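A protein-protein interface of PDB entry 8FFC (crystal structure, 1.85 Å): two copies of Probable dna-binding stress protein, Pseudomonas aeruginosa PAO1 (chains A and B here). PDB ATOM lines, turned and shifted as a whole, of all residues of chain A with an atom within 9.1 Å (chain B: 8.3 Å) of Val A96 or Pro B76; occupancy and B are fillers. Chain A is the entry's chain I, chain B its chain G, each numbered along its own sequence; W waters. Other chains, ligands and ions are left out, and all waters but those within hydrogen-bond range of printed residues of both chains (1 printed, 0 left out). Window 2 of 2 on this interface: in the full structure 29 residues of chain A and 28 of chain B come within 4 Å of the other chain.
Trp A38 touches Ala B67 (CE2 to CB, 3.2 Å). Trp A38 touches Glu B68 (CD1 to CG, 3.8 Å). Ala B77 touches Trp A38. O of Pro B78 touches CZ3 of Trp A38, at 3.6 Å. Arg B71 touches Asn A39 (CD to OD1, 3.4 Å). OD1 of Asn A39 touches CA of Pro B76 (3.3 Å). CG2 of Thr A41 touches NH2 of Arg B71, at 3.6 Å. CG2 of Val A96 touches CB of Pro B76, 3.8 Å away.
Hydrophobic or aromatic side chains of chain A that line the printed part of chain B: Trp A38 and Val A96. Of the 18 printed residues of chain B, 7 touch a printed residue of chain A. Printed residues of chain B that touch a printed residue of chain A: Ala B67, Glu B68, Arg B71, Pro B76, Ala B77, Pro B78 and Gly B79. Along chain B the printed residues that touch a printed residue of chain A span positions 67 to 79. Among the printed residues, 11 pairs touch across the chains. Among the printed residues, no Asp or Glu carboxylate lies within 4 Å of a Lys or Arg side-chain nitrogen of the other chain.
The backbone carbonyl oxygen (O) of Phe B75 sits at hydrogen-bond distance from the guanidinium group (NH1) of Arg B71 (3.0 Å). The side-chain amide nitrogen of Asn A39 lies within hydrogen-bond range of the side-chain amide oxygen of Asn A35 (3.0 Å).
Water W1 lies within hydrogen-bond range of O of Val A40 (2.7 Å), O of Trp A38 (2.9 Å) and NH2 of Arg B71 (2.9 Å).
No position is printed for both chains. Of the 11 pairs that touch across the chains among the printed residues, none has its exchanged pair printed and touching as well.
The guanidinium group of Arg B71 lies within hydrogen-bond range of the backbone carbonyl oxygen of Trp A38 (2.9 Å). O of Ala B77 lies within hydrogen-bond range of ND2 of Asn A39. The side-chain amide nitrogen (ND2) of Asn A35 is in hydrogen-bond range of the backbone carbonyl oxygen (O) of Gly B79, 3.1 Å away.
Of the printed residues of chain B, Trp A38 touches Ala B67, Glu B68, Arg B71, Ala B77 and Pro B78. Val A96 touches just one residue of chain B: Pro B76 (3.8 Å). Printed residues of chain A within 4 Å of Ala B67: Trp A38. Ala B72 touches none of the printed residues of chain A. Printed residues of chain A within 4 Å of Gly B79: Asn A35 (3.1 Å). The nearest printed residue of chain B that does not touch Asn A35 is Ala B77 (4.6 Å).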
ATOM      1  N   ASN A  35     -12.399 -19.788 -25.140  1.00  0.00           N
ATOM      2  CA  ASN A  35     -12.311 -21.068 -25.834  1.00  0.00           C
ATOM      3  C   ASN A  35     -10.968 -21.724 -25.573  1.00  0.00           C
ATOM      4  O   ASN A  35     -10.894 -22.879 -25.136  1.00  0.00           O
ATOM      5  CB  ASN A  35     -12.538 -20.808 -27.333  1.00  0.00           C
ATOM      6  CG  ASN A  35     -12.339 -22.003 -28.198  1.00  0.00           C
ATOM      7  OD1 ASN A  35     -11.509 -22.877 -27.934  1.00  0.00           O
ATOM      8  ND2 ASN A  35     -13.088 -22.025 -29.305  1.00  0.00           N
ATOM      9  N   PHE A  36      -9.890 -20.984 -25.792  1.00  0.00           N
ATOM     10  CA  PHE A  36      -8.578 -21.562 -25.575  1.00  0.00           C
ATOM     11  C   PHE A  36      -8.374 -21.923 -24.097  1.00  0.00           C
ATOM     12  O   PHE A  36      -7.675 -22.883 -23.791  1.00  0.00           O
ATOM     13  CB  PHE A  36      -7.495 -20.605 -26.063  1.00  0.00           C
ATOM     14  CG  PHE A  36      -7.447 -20.408 -27.582  1.00  0.00           C
ATOM     15  CD1 PHE A  36      -8.237 -21.159 -28.455  1.00  0.00           C
ATOM     16  CD2 PHE A  36      -6.584 -19.472 -28.124  1.00  0.00           C
ATOM     17  CE1 PHE A  36      -8.172 -20.952 -29.814  1.00  0.00           C
ATOM     18  CE2 PHE A  36      -6.512 -19.283 -29.481  1.00  0.00           C
ATOM     19  CZ  PHE A  36      -7.292 -20.029 -30.328  1.00  0.00           C
ATOM     20  N   TRP A  38     -10.597 -23.221 -22.095  1.00  0.00           N
ATOM     21  CA  TRP A  38     -11.168 -24.561 -21.897  1.00  0.00           C
ATOM     22  C   TRP A  38     -10.356 -25.634 -22.599  1.00  0.00           C
ATOM     23  O   TRP A  38     -10.239 -26.755 -22.098  1.00  0.00           O
ATOM     24  CB  TRP A  38     -12.597 -24.637 -22.437  1.00  0.00           C
ATOM     25  CG  TRP A  38     -13.554 -23.698 -21.851  1.00  0.00           C
ATOM     26  CD1 TRP A  38     -13.667 -23.338 -20.545  1.00  0.00           C
ATOM     27  CD2 TRP A  38     -14.570 -22.979 -22.559  1.00  0.00           C
ATOM     28  NE1 TRP A  38     -14.668 -22.410 -20.399  1.00  0.00           N
ATOM     29  CE2 TRP A  38     -15.244 -22.185 -21.624  1.00  0.00           C
ATOM     30  CE3 TRP A  38     -14.964 -22.926 -23.902  1.00  0.00           C
ATOM     31  CZ2 TRP A  38     -16.311 -21.353 -21.978  1.00  0.00           C
ATOM     32  CZ3 TRP A  38     -16.019 -22.084 -24.253  1.00  0.00           C
ATOM     33  CH2 TRP A  38     -16.670 -21.313 -23.302  1.00  0.00           C
ATOM     34  N   ASN A  39      -9.829 -25.339 -23.784  1.00  0.00           N
ATOM     35  CA  ASN A  39      -9.402 -26.389 -24.701  1.00  0.00           C
ATOM     36  C   ASN A  39      -7.896 -26.616 -24.804  1.00  0.00           C
ATOM     37  O   ASN A  39      -7.491 -27.601 -25.426  1.00  0.00           O
ATOM     38  CB  ASN A  39      -9.964 -26.078 -26.086  1.00  0.00           C
ATOM     39  CG  ASN A  39     -11.443 -26.401 -26.181  1.00  0.00           C
ATOM     40  OD1 ASN A  39     -11.857 -27.513 -25.869  1.00  0.00           O
ATOM     41  ND2 ASN A  39     -12.241 -25.437 -26.594  1.00  0.00           N
ATOM     42  N   VAL A  40      -7.062 -25.751 -24.216  1.00  0.00           N
ATOM     43  CA  VAL A  40      -5.611 -25.911 -24.296  1.00  0.00           C
ATOM     44  C   VAL A  40      -5.198 -27.184 -23.567  1.00  0.00           C
ATOM     45  O   VAL A  40      -5.771 -27.540 -22.539  1.00  0.00           O
ATOM     46  CB  VAL A  40      -4.895 -24.688 -23.686  1.00  0.00           C
ATOM     47  CG1 VAL A  40      -5.232 -24.523 -22.217  1.00  0.00           C
ATOM     48  CG2 VAL A  40      -3.386 -24.730 -23.919  1.00  0.00           C
ATOM     49  N   THR A  41      -4.162 -27.848 -24.071  1.00  0.00           N
ATOM     50  CA  THR A  41      -3.585 -29.001 -23.373  1.00  0.00           C
ATOM     51  C   THR A  41      -2.088 -29.003 -23.573  1.00  0.00           C
ATOM     52  O   THR A  41      -1.538 -28.220 -24.350  1.00  0.00           O
ATOM     53  CB  THR A  41      -4.159 -30.336 -23.855  1.00  0.00           C
ATOM     54  OG1 THR A  41      -3.867 -30.501 -25.241  1.00  0.00           O
ATOM     55  CG2 THR A  41      -5.645 -30.400 -23.639  1.00  0.00           C
ATOM     56  N   GLU A  93     -11.232 -19.195 -34.440  1.00  0.00           N
ATOM     57  CA  GLU A  93     -10.593 -20.497 -34.601  1.00  0.00           C
ATOM     58  C   GLU A  93     -11.663 -21.545 -34.338  1.00  0.00           C
ATOM     59  O   GLU A  93     -12.208 -21.597 -33.231  1.00  0.00           O
ATOM     60  CB  GLU A  93      -9.420 -20.654 -33.621  1.00  0.00           C
ATOM     61  CG  GLU A  93      -8.853 -22.058 -33.512  1.00  0.00           C
ATOM     62  CD  GLU A  93      -8.335 -22.579 -34.834  1.00  0.00           C
ATOM     63  OE1 GLU A  93      -7.451 -21.920 -35.429  1.00  0.00           O
ATOM     64  OE2 GLU A  93      -8.825 -23.639 -35.288  1.00  0.00           O
ATOM     65  N   GLU A  94     -12.006 -22.346 -35.369  1.00  0.00           N
ATOM     66  CA  GLU A  94     -13.094 -23.320 -35.241  1.00  0.00           C
ATOM     67  C   GLU A  94     -12.629 -24.675 -34.725  1.00  0.00           C
ATOM     68  O   GLU A  94     -13.473 -25.484 -34.332  1.00  0.00           O
ATOM     69  CB  GLU A  94     -13.823 -23.525 -36.590  1.00  0.00           C
ATOM     70  CG  GLU A  94     -14.433 -22.252 -37.212  1.00  0.00           C
ATOM     71  CD  GLU A  94     -15.546 -21.646 -36.377  1.00  0.00           C
ATOM     72  OE1 GLU A  94     -16.281 -22.409 -35.707  1.00  0.00           O
ATOM     73  OE2 GLU A  94     -15.699 -20.399 -36.400  1.00  0.00           O
ATOM     74  N   GLY A  95     -11.317 -24.925 -34.678  1.00  0.00           N
ATOM     75  CA  GLY A  95     -10.786 -26.167 -34.147  1.00  0.00           C
ATOM     76  C   GLY A  95     -10.053 -26.039 -32.822  1.00  0.00           C
ATOM     77  O   GLY A  95     -10.386 -25.161 -32.026  1.00  0.00           O
ATOM     78  N   VAL A  96      -9.070 -26.909 -32.574  1.00  0.00           N
ATOM     79  CA  VAL A  96      -8.328 -26.932 -31.311  1.00  0.00           C
ATOM     80  C   VAL A  96      -6.843 -26.942 -31.643  1.00  0.00           C
ATOM     81  O   VAL A  96      -6.247 -28.019 -31.821  1.00  0.00           O
ATOM     82  CB  VAL A  96      -8.700 -28.140 -30.437  1.00  0.00           C
ATOM     83  CG1 VAL A  96      -7.894 -28.114 -29.148  1.00  0.00           C
ATOM     84  CG2 VAL A  96     -10.162 -28.128 -30.125  1.00  0.00           C
ATOM     85  N   PRO A  97      -6.205 -25.780 -31.763  1.00  0.00           N
ATOM     86  CA  PRO A  97      -4.797 -25.759 -32.150  1.00  0.00           C
ATOM     87  C   PRO A  97      -3.918 -26.192 -30.992  1.00  0.00           C
ATOM     88  O   PRO A  97      -4.342 -26.243 -29.839  1.00  0.00           O
ATOM     89  CB  PRO A  97      -4.533 -24.295 -32.514  1.00  0.00           C
ATOM     90  CG  PRO A  97      -5.872 -23.642 -32.594  1.00  0.00           C
ATOM     91  CD  PRO A  97      -6.787 -24.425 -31.711  1.00  0.00           C
ATOM     92  N   GLU A  98      -2.664 -26.461 -31.325  1.00  0.00           N
ATOM     93  CA  GLU A  98      -1.640 -26.685 -30.314  1.00  0.00           C
ATOM     94  C   GLU A  98      -1.406 -25.406 -29.512  1.00  0.00           C
ATOM     95  O   GLU A  98      -1.708 -24.295 -29.958  1.00  0.00           O
ATOM     96  CB  GLU A  98      -0.335 -27.153 -30.973  1.00  0.00           C
ATOM     97  CG  GLU A  98      -0.409 -28.570 -31.599  1.00  0.00           C
ATOM     98  CD  GLU A  98      -0.522 -29.683 -30.556  1.00  0.00           C
ATOM     99  OE1 GLU A  98       0.533 -30.168 -30.094  1.00  0.00           O
ATOM    100  OE2 GLU A  98      -1.659 -30.064 -30.184  1.00  0.00           O
ATOM    101  N   ALA A  99      -0.856 -25.575 -28.310  1.00  0.00           N
ATOM    102  CA  ALA A  99      -0.782 -24.464 -27.366  1.00  0.00           C
ATOM    103  C   ALA A  99       0.003 -23.288 -27.935  1.00  0.00           C
ATOM    104  O   ALA A  99      -0.400 -22.130 -27.767  1.00  0.00           O
ATOM    105  CB  ALA A  99      -0.155 -24.949 -26.063  1.00  0.00           C
ATOM    106  N   GLU A 101       0.365 -22.369 -31.017  1.00  0.00           N
ATOM    107  CA  GLU A 101      -0.458 -21.661 -31.985  1.00  0.00           C
ATOM    108  C   GLU A 101      -1.580 -20.885 -31.309  1.00  0.00           C
ATOM    109  O   GLU A 101      -1.961 -19.814 -31.786  1.00  0.00           O
ATOM    110  CB  GLU A 101      -1.023 -22.646 -33.004  1.00  0.00           C
ATOM    111  CG  GLU A 101      -2.096 -22.064 -33.925  1.00  0.00           C
ATOM    112  CD  GLU A 101      -1.578 -20.962 -34.870  1.00  0.00           C
ATOM    113  OE1 GLU A 101      -0.338 -20.763 -34.986  1.00  0.00           O
ATOM    114  OE2 GLU A 101      -2.433 -20.301 -35.510  1.00  0.00           O
ATOM    115  N   MET A 102      -2.149 -21.408 -30.219  1.00  0.00           N
ATOM    116  CA  MET A 102      -3.107 -20.609 -29.456  1.00  0.00           C
ATOM    117  C   MET A 102      -2.449 -19.325 -28.977  1.00  0.00           C
ATOM    118  O   MET A 102      -3.019 -18.236 -29.091  1.00  0.00           O
ATOM    119  CB  MET A 102      -3.663 -21.387 -28.257  1.00  0.00           C
ATOM    120  CG  MET A 102      -4.635 -22.500 -28.634  1.00  0.00           C
ATOM    121  SD  MET A 102      -5.141 -23.382 -27.139  1.00  0.00           S
ATOM    122  CE  MET A 102      -6.477 -24.444 -27.748  1.00  0.00           C
ATOM    123  N   GLN A 105      -2.029 -16.942 -31.896  1.00  0.00           N
ATOM    124  CA  GLN A 105      -3.280 -16.301 -32.296  1.00  0.00           C
ATOM    125  C   GLN A 105      -3.699 -15.233 -31.290  1.00  0.00           C
ATOM    126  O   GLN A 105      -4.268 -14.207 -31.673  1.00  0.00           O
ATOM    127  CB  GLN A 105      -4.413 -17.319 -32.460  1.00  0.00           C
ATOM    128  CG  GLN A 105      -4.342 -18.134 -33.717  1.00  0.00           C
ATOM    129  CD  GLN A 105      -5.599 -18.959 -33.937  1.00  0.00           C
ATOM    130  OE1 GLN A 105      -6.714 -18.529 -33.634  1.00  0.00           O
ATOM    131  NE2 GLN A 105      -5.414 -20.149 -34.482  1.00  0.00           N
ATOM    132  N   ALA B  16     -21.735 -35.200 -24.238  1.00  0.00           N
ATOM    133  CA  ALA B  16     -21.055 -33.966 -24.627  1.00  0.00           C
ATOM    134  C   ALA B  16     -21.818 -33.230 -25.713  1.00  0.00           C
ATOM    135  O   ALA B  16     -21.821 -31.990 -25.748  1.00  0.00           O
ATOM    136  CB  ALA B  16     -19.646 -34.287 -25.116  1.00  0.00           C
ATOM    137  N   GLU B  17     -22.479 -33.970 -26.604  1.00  0.00           N
ATOM    138  CA  GLU B  17     -23.281 -33.330 -27.639  1.00  0.00           C
ATOM    139  C   GLU B  17     -24.463 -32.602 -27.027  1.00  0.00           C
ATOM    140  O   GLU B  17     -24.784 -31.478 -27.430  1.00  0.00           O
ATOM    141  CB  GLU B  17     -23.749 -34.372 -28.671  1.00  0.00           C
ATOM    142  CG  GLU B  17     -24.445 -33.770 -29.884  1.00  0.00           C
ATOM    143  CD  GLU B  17     -25.828 -33.139 -29.598  1.00  0.00           C
ATOM    144  OE1 GLU B  17     -26.657 -33.730 -28.852  1.00  0.00           O
ATOM    145  OE2 GLU B  17     -26.086 -32.036 -30.137  1.00  0.00           O
ATOM    146  N   SER B  20     -23.258 -29.561 -25.346  1.00  0.00           N
ATOM    147  CA  SER B  20     -22.908 -28.549 -26.341  1.00  0.00           C
ATOM    148  C   SER B  20     -24.121 -27.700 -26.716  1.00  0.00           C
ATOM    149  O   SER B  20     -24.022 -26.471 -26.826  1.00  0.00           O
ATOM    150  CB  SER B  20     -22.292 -29.206 -27.566  1.00  0.00           C
ATOM    151  OG  SER B  20     -20.984 -29.669 -27.295  1.00  0.00           O
ATOM    152  N   LEU B  23     -24.637 -25.489 -23.661  1.00  0.00           N
ATOM    153  CA  LEU B  23     -23.650 -24.411 -23.650  1.00  0.00           C
ATOM    154  C   LEU B  23     -24.029 -23.331 -24.652  1.00  0.00           C
ATOM    155  O   LEU B  23     -24.016 -22.146 -24.338  1.00  0.00           O
ATOM    156  CB  LEU B  23     -22.275 -24.986 -23.963  1.00  0.00           C
ATOM    157  CG  LEU B  23     -21.088 -24.007 -24.070  1.00  0.00           C
ATOM    158  CD1 LEU B  23     -20.909 -23.268 -22.804  1.00  0.00           C
ATOM    159  CD2 LEU B  23     -19.849 -24.762 -24.421  1.00  0.00           C
ATOM    160  N   ILE B  66     -20.319 -25.391 -17.706  1.00  0.00           N
ATOM    161  CA  ILE B  66     -20.808 -26.337 -18.719  1.00  0.00           C
ATOM    162  C   ILE B  66     -19.669 -26.776 -19.623  1.00  0.00           C
ATOM    163  O   ILE B  66     -19.461 -27.973 -19.873  1.00  0.00           O
ATOM    164  CB  ILE B  66     -21.972 -25.716 -19.517  1.00  0.00           C
ATOM    165  CG1 ILE B  66     -23.123 -25.385 -18.589  1.00  0.00           C
ATOM    166  CG2 ILE B  66     -22.415 -26.682 -20.629  1.00  0.00           C
ATOM    167  CD1 ILE B  66     -24.174 -24.427 -19.148  1.00  0.00           C
ATOM    168  N   ALA B  67     -18.885 -25.812 -20.104  1.00  0.00           N
ATOM    169  CA  ALA B  67     -17.779 -26.138 -20.995  1.00  0.00           C
ATOM    170  C   ALA B  67     -16.797 -27.096 -20.335  1.00  0.00           C
ATOM    171  O   ALA B  67     -16.277 -28.021 -20.974  1.00  0.00           O
ATOM    172  CB  ALA B  67     -17.058 -24.848 -21.406  1.00  0.00           C
ATOM    173  N   GLU B  68     -16.529 -26.889 -19.053  1.00  0.00           N
ATOM    174  CA  GLU B  68     -15.515 -27.701 -18.395  1.00  0.00           C
ATOM    175  C   GLU B  68     -16.049 -29.089 -18.047  1.00  0.00           C
ATOM    176  O   GLU B  68     -15.265 -30.044 -17.974  1.00  0.00           O
ATOM    177  CB  GLU B  68     -14.991 -26.958 -17.170  1.00  0.00           C
ATOM    178  CG  GLU B  68     -14.157 -25.750 -17.637  1.00  0.00           C
ATOM    179  CD  GLU B  68     -13.421 -25.000 -16.545  1.00  0.00           C
ATOM    180  OE1 GLU B  68     -13.628 -25.259 -15.346  1.00  0.00           O
ATOM    181  OE2 GLU B  68     -12.640 -24.106 -16.940  1.00  0.00           O
ATOM    182  N   ARG B  69     -17.361 -29.232 -17.907  1.00  0.00           N
ATOM    183  CA  ARG B  69     -17.919 -30.579 -17.812  1.00  0.00           C
ATOM    184  C   ARG B  69     -17.746 -31.335 -19.128  1.00  0.00           C
ATOM    185  O   ARG B  69     -17.371 -32.522 -19.131  1.00  0.00           O
ATOM    186  CB  ARG B  69     -19.390 -30.516 -17.404  1.00  0.00           C
ATOM    187  CG  ARG B  69     -20.039 -31.899 -17.255  1.00  0.00           C
ATOM    188  CD  ARG B  69     -19.329 -32.731 -16.197  1.00  0.00           C
ATOM    189  NE  ARG B  69     -19.844 -34.098 -16.124  1.00  0.00           N
ATOM    190  CZ  ARG B  69     -19.150 -35.105 -15.619  1.00  0.00           C
ATOM    191  NH1 ARG B  69     -17.954 -34.910 -15.081  1.00  0.00           N
ATOM    192  NH2 ARG B  69     -19.663 -36.337 -15.658  1.00  0.00           N
ATOM    193  N   ILE B  70     -17.972 -30.659 -20.261  1.00  0.00           N
ATOM    194  CA  ILE B  70     -17.661 -31.268 -21.550  1.00  0.00           C
ATOM    195  C   ILE B  70     -16.201 -31.710 -21.591  1.00  0.00           C
ATOM    196  O   ILE B  70     -15.881 -32.803 -22.076  1.00  0.00           O
ATOM    197  CB  ILE B  70     -17.989 -30.311 -22.720  1.00  0.00           C
ATOM    198  CG1 ILE B  70     -19.484 -30.047 -22.842  1.00  0.00           C
ATOM    199  CG2 ILE B  70     -17.452 -30.892 -24.039  1.00  0.00           C
ATOM    200  CD1 ILE B  70     -19.825 -28.887 -23.795  1.00  0.00           C
ATOM    201  N   ARG B  71     -15.271 -30.857 -21.119  1.00  0.00           N
ATOM    202  CA  ARG B  71     -13.866 -31.271 -21.122  1.00  0.00           C
ATOM    203  C   ARG B  71     -13.641 -32.502 -20.243  1.00  0.00           C
ATOM    204  O   ARG B  71     -12.854 -33.386 -20.595  1.00  0.00           O
ATOM    205  CB  ARG B  71     -12.945 -30.136 -20.641  1.00  0.00           C
ATOM    206  CG  ARG B  71     -12.938 -28.901 -21.524  1.00  0.00           C
ATOM    207  CD  ARG B  71     -12.401 -29.139 -22.894  1.00  0.00           C
ATOM    208  NE  ARG B  71     -10.990 -29.485 -22.866  1.00  0.00           N
ATOM    209  CZ  ARG B  71     -10.465 -30.650 -23.222  1.00  0.00           C
ATOM    210  NH1 ARG B  71     -11.205 -31.630 -23.725  1.00  0.00           N
ATOM    211  NH2 ARG B  71      -9.160 -30.842 -23.069  1.00  0.00           N
ATOM    212  N   ALA B  72     -14.254 -32.523 -19.064  1.00  0.00           N
ATOM    213  CA  ALA B  72     -14.109 -33.655 -18.150  1.00  0.00           C
ATOM    214  C   ALA B  72     -14.600 -34.957 -18.779  1.00  0.00           C
ATOM    215  O   ALA B  72     -14.055 -36.038 -18.489  1.00  0.00           O
ATOM    216  CB  ALA B  72     -14.885 -33.377 -16.866  1.00  0.00           C
ATOM    217  N   LEU B  73     -15.604 -34.873 -19.653  1.00  0.00           N
ATOM    218  CA  LEU B  73     -16.068 -36.051 -20.389  1.00  0.00           C
ATOM    219  C   LEU B  73     -15.159 -36.426 -21.541  1.00  0.00           C
ATOM    220  O   LEU B  73     -15.372 -37.477 -22.144  1.00  0.00           O
ATOM    221  CB  LEU B  73     -17.475 -35.832 -20.919  1.00  0.00           C
ATOM    222  CG  LEU B  73     -18.555 -35.761 -19.851  1.00  0.00           C
ATOM    223  CD1 LEU B  73     -19.719 -34.984 -20.362  1.00  0.00           C
ATOM    224  CD2 LEU B  73     -18.978 -37.151 -19.414  1.00  0.00           C
ATOM    225  N   GLY B  74     -14.175 -35.600 -21.874  1.00  0.00           N
ATOM    226  CA  GLY B  74     -13.147 -35.976 -22.815  1.00  0.00           C
ATOM    227  C   GLY B  74     -13.313 -35.405 -24.193  1.00  0.00           C
ATOM    228  O   GLY B  74     -12.769 -35.978 -25.152  1.00  0.00           O
ATOM    229  N   PHE B  75     -14.013 -34.285 -24.324  1.00  0.00           N
ATOM    230  CA  PHE B  75     -14.313 -33.724 -25.630  1.00  0.00           C
ATOM    231  C   PHE B  75     -14.033 -32.229 -25.638  1.00  0.00           C
ATOM    232  O   PHE B  75     -14.116 -31.577 -24.601  1.00  0.00           O
ATOM    233  CB  PHE B  75     -15.775 -34.004 -25.988  1.00  0.00           C
ATOM    234  CG  PHE B  75     -16.015 -35.463 -26.206  1.00  0.00           C
ATOM    235  CD1 PHE B  75     -15.704 -36.025 -27.426  1.00  0.00           C
ATOM    236  CD2 PHE B  75     -16.400 -36.292 -25.158  1.00  0.00           C
ATOM    237  CE1 PHE B  75     -15.844 -37.381 -27.628  1.00  0.00           C
ATOM    238  CE2 PHE B  75     -16.545 -37.660 -25.357  1.00  0.00           C
ATOM    239  CZ  PHE B  75     -16.262 -38.195 -26.592  1.00  0.00           C
ATOM    240  N   PRO B  76     -13.715 -31.664 -26.794  1.00  0.00           N
ATOM    241  CA  PRO B  76     -13.485 -30.211 -26.851  1.00  0.00           C
ATOM    242  C   PRO B  76     -14.775 -29.455 -26.649  1.00  0.00           C
ATOM    243  O   PRO B  76     -15.859 -29.906 -27.031  1.00  0.00           O
ATOM    244  CB  PRO B  76     -12.902 -29.994 -28.261  1.00  0.00           C
ATOM    245  CG  PRO B  76     -13.439 -31.117 -29.068  1.00  0.00           C
ATOM    246  CD  PRO B  76     -13.636 -32.294 -28.120  1.00  0.00           C
ATOM    247  N   ALA B  77     -14.662 -28.315 -26.018  1.00  0.00           N
ATOM    248  CA  ALA B  77     -15.837 -27.503 -25.811  1.00  0.00           C
ATOM    249  C   ALA B  77     -15.978 -26.520 -26.970  1.00  0.00           C
ATOM    250  O   ALA B  77     -14.993 -25.850 -27.325  1.00  0.00           O
ATOM    251  CB  ALA B  77     -15.742 -26.742 -24.497  1.00  0.00           C
ATOM    252  N   PRO B  78     -17.149 -26.433 -27.597  1.00  0.00           N
ATOM    253  CA  PRO B  78     -17.341 -25.445 -28.664  1.00  0.00           C
ATOM    254  C   PRO B  78     -17.316 -24.024 -28.121  1.00  0.00           C
ATOM    255  O   PRO B  78     -17.737 -23.747 -26.994  1.00  0.00           O
ATOM    256  CB  PRO B  78     -18.719 -25.800 -29.230  1.00  0.00           C
ATOM    257  CG  PRO B  78     -19.427 -26.414 -28.073  1.00  0.00           C
ATOM    258  CD  PRO B  78     -18.378 -27.212 -27.361  1.00  0.00           C
ATOM    259  N   GLY B  79     -16.859 -23.106 -28.976  1.00  0.00           N
ATOM    260  CA  GLY B  79     -16.578 -21.754 -28.532  1.00  0.00           C
ATOM    261  C   GLY B  79     -16.377 -20.760 -29.661  1.00  0.00           C
ATOM    262  O   GLY B  79     -15.372 -20.039 -29.687  1.00  0.00           O
HETATM  263  O   HOH W   1      -8.064 -28.585 -21.647  1.00  0.00           O
